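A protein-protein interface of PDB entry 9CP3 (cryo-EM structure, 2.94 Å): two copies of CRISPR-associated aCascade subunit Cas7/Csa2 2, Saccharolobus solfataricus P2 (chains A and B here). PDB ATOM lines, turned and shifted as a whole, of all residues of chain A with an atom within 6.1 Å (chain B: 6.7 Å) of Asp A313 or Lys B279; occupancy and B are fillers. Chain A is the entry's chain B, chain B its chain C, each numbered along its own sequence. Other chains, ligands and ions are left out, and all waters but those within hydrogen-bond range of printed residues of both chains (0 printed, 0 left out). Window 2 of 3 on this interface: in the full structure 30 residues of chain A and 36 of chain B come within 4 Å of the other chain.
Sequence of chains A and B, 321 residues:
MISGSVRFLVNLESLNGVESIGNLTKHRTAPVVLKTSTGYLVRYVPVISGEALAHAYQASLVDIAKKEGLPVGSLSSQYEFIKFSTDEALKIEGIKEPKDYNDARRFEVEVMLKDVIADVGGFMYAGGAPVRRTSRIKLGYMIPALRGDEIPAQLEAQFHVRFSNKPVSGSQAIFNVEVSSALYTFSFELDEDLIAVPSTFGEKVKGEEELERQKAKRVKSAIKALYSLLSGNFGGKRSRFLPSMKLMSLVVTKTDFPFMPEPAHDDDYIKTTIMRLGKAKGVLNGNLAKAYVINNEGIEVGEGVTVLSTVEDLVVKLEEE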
ATOM      1  N   LEU A 308      21.230  -8.120   7.180  1.00  0.00           N
ATOM      2  CA  LEU A 308      21.278  -9.048   8.300  1.00  0.00           C
ATOM      3  C   LEU A 308      20.680 -10.386   7.876  1.00  0.00           C
ATOM      4  O   LEU A 308      20.318 -10.595   6.716  1.00  0.00           O
ATOM      5  CB  LEU A 308      20.545  -8.469   9.510  1.00  0.00           C
ATOM      6  CG  LEU A 308      21.119  -7.174  10.085  1.00  0.00           C
ATOM      7  CD1 LEU A 308      20.050  -6.408  10.840  1.00  0.00           C
ATOM      8  CD2 LEU A 308      22.301  -7.472  10.990  1.00  0.00           C
ATOM      9  N   SER A 309      20.586 -11.297   8.828  1.00  0.00           N
ATOM     10  CA  SER A 309      20.020 -12.613   8.550  1.00  0.00           C
ATOM     11  C   SER A 309      18.869 -12.973   9.475  1.00  0.00           C
ATOM     12  O   SER A 309      17.895 -13.579   9.026  1.00  0.00           O
ATOM     13  CB  SER A 309      21.115 -13.685   8.647  1.00  0.00           C
ATOM     14  OG  SER A 309      21.783 -13.612   9.894  1.00  0.00           O
ATOM     15  N   THR A 310      18.960 -12.619  10.755  1.00  0.00           N
ATOM     16  CA  THR A 310      17.922 -12.946  11.726  1.00  0.00           C
ATOM     17  C   THR A 310      17.520 -11.706  12.512  1.00  0.00           C
ATOM     18  O   THR A 310      17.945 -10.592  12.191  1.00  0.00           O
ATOM     19  CB  THR A 310      18.393 -14.042  12.688  1.00  0.00           C
ATOM     20  OG1 THR A 310      19.500 -13.561  13.459  1.00  0.00           O
ATOM     21  CG2 THR A 310      18.812 -15.292  11.927  1.00  0.00           C
ATOM     22  N   VAL A 311      16.698 -11.894  13.540  1.00  0.00           N
ATOM     23  CA  VAL A 311      16.211 -10.771  14.331  1.00  0.00           C
ATOM     24  C   VAL A 311      17.082 -10.552  15.566  1.00  0.00           C
ATOM     25  O   VAL A 311      17.235  -9.413  16.023  1.00  0.00           O
ATOM     26  CB  VAL A 311      14.741 -10.997  14.719  1.00  0.00           C
ATOM     27  CG1 VAL A 311      14.214  -9.830  15.531  1.00  0.00           C
ATOM     28  CG2 VAL A 311      13.897 -11.204  13.474  1.00  0.00           C
ATOM     29  N   GLU A 312      17.661 -11.624  16.111  1.00  0.00           N
ATOM     30  CA  GLU A 312      18.503 -11.496  17.295  1.00  0.00           C
ATOM     31  C   GLU A 312      19.724 -10.635  17.002  1.00  0.00           C
ATOM     32  O   GLU A 312      20.164  -9.855  17.856  1.00  0.00           O
ATOM     33  CB  GLU A 312      18.921 -12.880  17.789  1.00  0.00           C
ATOM     34  CG  GLU A 312      17.759 -13.739  18.257  1.00  0.00           C
ATOM     35  CD  GLU A 312      17.129 -14.529  17.128  1.00  0.00           C
ATOM     36  OE1 GLU A 312      17.572 -14.369  15.971  1.00  0.00           O
ATOM     37  OE2 GLU A 312      16.187 -15.305  17.392  1.00  0.00           O
ATOM     38  N   ASP A 313      20.291 -10.771  15.802  1.00  0.00           N
ATOM     39  CA  ASP A 313      21.394  -9.904  15.405  1.00  0.00           C
ATOM     40  C   ASP A 313      20.957  -8.446  15.375  1.00  0.00           C
ATOM     41  O   ASP A 313      21.705  -7.556  15.798  1.00  0.00           O
ATOM     42  CB  ASP A 313      21.933 -10.330  14.041  1.00  0.00           C
ATOM     43  CG  ASP A 313      22.902 -11.487  14.136  1.00  0.00           C
ATOM     44  OD1 ASP A 313      23.350 -11.796  15.261  1.00  0.00           O
ATOM     45  OD2 ASP A 313      23.222 -12.083  13.087  1.00  0.00           O
ATOM     46  N   LEU A 314      19.747  -8.183  14.877  1.00  0.00           N
ATOM     47  CA  LEU A 314      19.230  -6.819  14.876  1.00  0.00           C
ATOM     48  C   LEU A 314      19.087  -6.286  16.294  1.00  0.00           C
ATOM     49  O   LEU A 314      19.427  -5.130  16.567  1.00  0.00           O
ATOM     50  CB  LEU A 314      17.887  -6.767  14.150  1.00  0.00           C
ATOM     51  CG  LEU A 314      17.195  -5.403  14.128  1.00  0.00           C
ATOM     52  CD1 LEU A 314      17.762  -4.528  13.024  1.00  0.00           C
ATOM     53  CD2 LEU A 314      15.689  -5.556  13.980  1.00  0.00           C
ATOM     54  N   VAL A 315      18.585  -7.116  17.212  1.00  0.00           N
ATOM     55  CA  VAL A 315      18.432  -6.680  18.598  1.00  0.00           C
ATOM     56  C   VAL A 315      19.793  -6.377  19.216  1.00  0.00           C
ATOM     57  O   VAL A 315      19.963  -5.373  19.919  1.00  0.00           O
ATOM     58  CB  VAL A 315      17.662  -7.738  19.409  1.00  0.00           C
ATOM     59  CG1 VAL A 315      17.509  -7.290  20.851  1.00  0.00           C
ATOM     60  CG2 VAL A 315      16.302  -7.993  18.785  1.00  0.00           C
ATOM     61  N   VAL A 316      20.782  -7.236  18.960  1.00  0.00           N
ATOM     62  CA  VAL A 316      22.122  -7.012  19.501  1.00  0.00           C
ATOM     63  C   VAL A 316      22.707  -5.715  18.958  1.00  0.00           C
ATOM     64  O   VAL A 316      23.289  -4.919  19.705  1.00  0.00           O
ATOM     65  CB  VAL A 316      23.031  -8.217  19.195  1.00  0.00           C
ATOM     66  CG1 VAL A 316      24.487  -7.863  19.445  1.00  0.00           C
ATOM     67  CG2 VAL A 316      22.627  -9.411  20.038  1.00  0.00           C
ATOM     68  N   LYS A 317      22.566  -5.485  17.651  1.00  0.00           N
ATOM     69  CA  LYS A 317      23.110  -4.270  17.051  1.00  0.00           C
ATOM     70  C   LYS A 317      22.413  -3.028  17.589  1.00  0.00           C
ATOM     71  O   LYS A 317      23.054  -1.994  17.807  1.00  0.00           O
ATOM     72  CB  LYS A 317      22.997  -4.339  15.528  1.00  0.00           C
ATOM     73  CG  LYS A 317      24.003  -5.274  14.884  1.00  0.00           C
ATOM     74  CD  LYS A 317      24.022  -5.108  13.378  1.00  0.00           C
ATOM     75  CE  LYS A 317      24.982  -4.007  12.966  1.00  0.00           C
ATOM     76  NZ  LYS A 317      26.382  -4.327  13.357  1.00  0.00           N
ATOM     77  N   LEU A 318      21.096  -3.105  17.799  1.00  0.00           N
ATOM     78  CA  LEU A 318      20.377  -1.976  18.378  1.00  0.00           C
ATOM     79  C   LEU A 318      20.837  -1.704  19.805  1.00  0.00           C
ATOM     80  O   LEU A 318      20.958  -0.543  20.213  1.00  0.00           O
ATOM     81  CB  LEU A 318      18.874  -2.241  18.344  1.00  0.00           C
ATOM     82  CG  LEU A 318      18.180  -2.077  16.992  1.00  0.00           C
ATOM     83  CD1 LEU A 318      16.849  -2.810  16.986  1.00  0.00           C
ATOM     84  CD2 LEU A 318      17.987  -0.612  16.666  1.00  0.00           C
ATOM     85  N   ILE B 274      18.362 -23.707  15.156  1.00  0.00           N
ATOM     86  CA  ILE B 274      19.487 -23.864  16.077  1.00  0.00           C
ATOM     87  C   ILE B 274      20.240 -22.547  16.243  1.00  0.00           C
ATOM     88  O   ILE B 274      20.587 -22.144  17.364  1.00  0.00           O
ATOM     89  CB  ILE B 274      20.411 -24.991  15.588  1.00  0.00           C
ATOM     90  CG1 ILE B 274      19.762 -26.349  15.852  1.00  0.00           C
ATOM     91  CG2 ILE B 274      21.771 -24.903  16.260  1.00  0.00           C
ATOM     92  CD1 ILE B 274      20.077 -27.383  14.803  1.00  0.00           C
ATOM     93  N   MET B 275      20.513 -21.861  15.130  1.00  0.00           N
ATOM     94  CA  MET B 275      21.211 -20.581  15.204  1.00  0.00           C
ATOM     95  C   MET B 275      20.387 -19.558  15.970  1.00  0.00           C
ATOM     96  O   MET B 275      20.917 -18.814  16.808  1.00  0.00           O
ATOM     97  CB  MET B 275      21.523 -20.071  13.797  1.00  0.00           C
ATOM     98  CG  MET B 275      22.479 -20.951  13.011  1.00  0.00           C
ATOM     99  SD  MET B 275      24.166 -20.885  13.643  1.00  0.00           S
ATOM    100  CE  MET B 275      24.305 -22.498  14.409  1.00  0.00           C
ATOM    101  N   ARG B 276      19.080 -19.513  15.699  1.00  0.00           N
ATOM    102  CA  ARG B 276      18.211 -18.592  16.418  1.00  0.00           C
ATOM    103  C   ARG B 276      18.175 -18.922  17.903  1.00  0.00           C
ATOM    104  O   ARG B 276      18.144 -18.019  18.742  1.00  0.00           O
ATOM    105  CB  ARG B 276      16.805 -18.630  15.824  1.00  0.00           C
ATOM    106  CG  ARG B 276      16.541 -17.550  14.792  1.00  0.00           C
ATOM    107  CD  ARG B 276      15.161 -17.707  14.183  1.00  0.00           C
ATOM    108  NE  ARG B 276      14.119 -17.186  15.058  1.00  0.00           N
ATOM    109  CZ  ARG B 276      13.198 -17.934  15.649  1.00  0.00           C
ATOM    110  NH1 ARG B 276      13.160 -19.245  15.477  1.00  0.00           N
ATOM    111  NH2 ARG B 276      12.293 -17.353  16.432  1.00  0.00           N
ATOM    112  N   LEU B 277      18.189 -20.212  18.247  1.00  0.00           N
ATOM    113  CA  LEU B 277      18.184 -20.610  19.649  1.00  0.00           C
ATOM    114  C   LEU B 277      19.452 -20.162  20.358  1.00  0.00           C
ATOM    115  O   LEU B 277      19.396 -19.634  21.475  1.00  0.00           O
ATOM    116  CB  LEU B 277      18.025 -22.125  19.759  1.00  0.00           C
ATOM    117  CG  LEU B 277      18.026 -22.675  21.183  1.00  0.00           C
ATOM    118  CD1 LEU B 277      16.715 -22.330  21.845  1.00  0.00           C
ATOM    119  CD2 LEU B 277      18.251 -24.176  21.178  1.00  0.00           C
ATOM    120  N   GLY B 278      20.608 -20.363  19.723  1.00  0.00           N
ATOM    121  CA  GLY B 278      21.849 -19.911  20.331  1.00  0.00           C
ATOM    122  C   GLY B 278      21.879 -18.407  20.525  1.00  0.00           C
ATOM    123  O   GLY B 278      22.237 -17.905  21.598  1.00  0.00           O
ATOM    124  N   LYS B 279      21.477 -17.664  19.492  1.00  0.00           N
ATOM    125  CA  LYS B 279      21.496 -16.208  19.592  1.00  0.00           C
ATOM    126  C   LYS B 279      20.487 -15.702  20.617  1.00  0.00           C
ATOM    127  O   LYS B 279      20.757 -14.729  21.328  1.00  0.00           O
ATOM    128  CB  LYS B 279      21.245 -15.589  18.220  1.00  0.00           C
ATOM    129  CG  LYS B 279      22.489 -15.531  17.348  1.00  0.00           C
ATOM    130  CD  LYS B 279      22.207 -14.871  16.012  1.00  0.00           C
ATOM    131  CE  LYS B 279      23.359 -15.080  15.043  1.00  0.00           C
ATOM    132  NZ  LYS B 279      23.401 -16.474  14.531  1.00  0.00           N
ATOM    133  N   ALA B 280      19.327 -16.354  20.724  1.00  0.00           N
ATOM    134  CA  ALA B 280      18.338 -15.945  21.715  1.00  0.00           C
ATOM    135  C   ALA B 280      18.796 -16.265  23.131  1.00  0.00           C
ATOM    136  O   ALA B 280      18.516 -15.503  24.063  1.00  0.00           O
ATOM    137  CB  ALA B 280      16.996 -16.614  21.423  1.00  0.00           C
ATOM    138  N   LYS B 281      19.484 -17.395  23.321  1.00  0.00           N
ATOM    139  CA  LYS B 281      20.065 -17.679  24.629  1.00  0.00           C
ATOM    140  C   LYS B 281      21.102 -16.630  24.998  1.00  0.00           C
ATOM    141  O   LYS B 281      21.178 -16.200  26.155  1.00  0.00           O
ATOM    142  CB  LYS B 281      20.684 -19.075  24.651  1.00  0.00           C
ATOM    143  CG  LYS B 281      21.088 -19.527  26.045  1.00  0.00           C
ATOM    144  CD  LYS B 281      22.322 -20.406  26.016  1.00  0.00           C
ATOM    145  CE  LYS B 281      22.733 -20.808  27.421  1.00  0.00           C
ATOM    146  NZ  LYS B 281      23.649 -21.979  27.419  1.00  0.00           N
ATOM    147  N   GLY B 282      21.913 -16.210  24.026  1.00  0.00           N
ATOM    148  CA  GLY B 282      22.852 -15.129  24.287  1.00  0.00           C
ATOM    149  C   GLY B 282      22.160 -13.822  24.630  1.00  0.00           C
ATOM    150  O   GLY B 282      22.590 -13.098  25.530  1.00  0.00           O
ATOM    151  N   VAL B 283      21.077 -13.506  23.916  1.00  0.00           N
ATOM    152  CA  VAL B 283      20.406 -12.220  24.094  1.00  0.00           C
ATOM    153  C   VAL B 283      19.688 -12.165  25.437  1.00  0.00           C
ATOM    154  O   VAL B 283      19.801 -11.183  26.180  1.00  0.00           O
ATOM    155  CB  VAL B 283      19.434 -11.964  22.929  1.00  0.00           C
ATOM    156  CG1 VAL B 283      18.398 -10.918  23.314  1.00  0.00           C
ATOM    157  CG2 VAL B 283      20.191 -11.538  21.686  1.00  0.00           C
ATOM    158  N   LEU B 284      18.943 -13.215  25.770  1.00  0.00           N
ATOM    159  CA  LEU B 284      18.032 -13.203  26.907  1.00  0.00           C
ATOM    160  C   LEU B 284      18.677 -13.681  28.201  1.00  0.00           C
ATOM    161  O   LEU B 284      17.977 -13.804  29.213  1.00  0.00           O
ATOM    162  CB  LEU B 284      16.802 -14.061  26.599  1.00  0.00           C
ATOM    163  CG  LEU B 284      15.871 -13.529  25.509  1.00  0.00           C
ATOM    164  CD1 LEU B 284      14.914 -14.613  25.040  1.00  0.00           C
ATOM    165  CD2 LEU B 284      15.102 -12.318  26.014  1.00  0.00           C
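Printed residues of chain B within 4 Å of Thr A310: Lys B279.
Of chain B, only Lys B279 comes within 4 Å of Asp A313.
Printed residues of chain B within 4 Å of Val A316: Val B283.
Printed residues of chain A within 4 Å of Arg B276: Glu A312.
Of chain A, only Thr A310, Glu A312 and Asp A313 come within 4 Å of Lys B279.
Of the printed residues of chain A, Ala B280 touches Glu A312 (3.9 Å).
Lys B281 touches none of the printed residues of chain A.
Of the printed residues of chain A, Val B283 touches Val A316 (3.6 Å).
Leu B284 touches none of the printed residues of chain A.
The nearest residue of chain B that does not touch Asp A313 is Val B283 (5.9 Å).
The nearest residue of chain A that does not touch Lys B279 is Ser A309 (5.6 Å).
The side-chain carboxylate (OE2) of Glu A312 lies within salt-bridge range of the guanidinium group (NE) of Arg B276.
No position is printed for both chains.
Printed residues of chain B that touch a printed residue of chain A: Arg B276, Lys B279, Ala B280 and Val B283.
Hydrophobic or aromatic side chains of chain B within 4 Å of the printed part of chain A: Val B283.
Along chain B the printed residues that touch a printed residue of chain A span positions 276 to 283.
Of the 11 printed residues of chain A, 4 touch a printed residue of chain B.
Printed residues of chain A that touch a printed residue of chain B: Thr A310, Glu A312, Asp A313 and Val A316.
Among the printed residues, 6 pairs touch across the chains.
The side-chain carboxylate (OE1) of Glu A312 lies within hydrogen-bond range of the side-chain hydroxyl (OG1) of Thr A310 (3.3 Å).
Among the printed residues, merely in contact across the chains: Asp A313 with Lys B279 (3.3 Å), Glu A312 with Lys B279 (3.6 Å), Val A316 with Val B283 (3.6 Å), Glu A312 with Ala B280 (3.9 Å) and Thr A310 with Lys B279 (3.9 Å).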
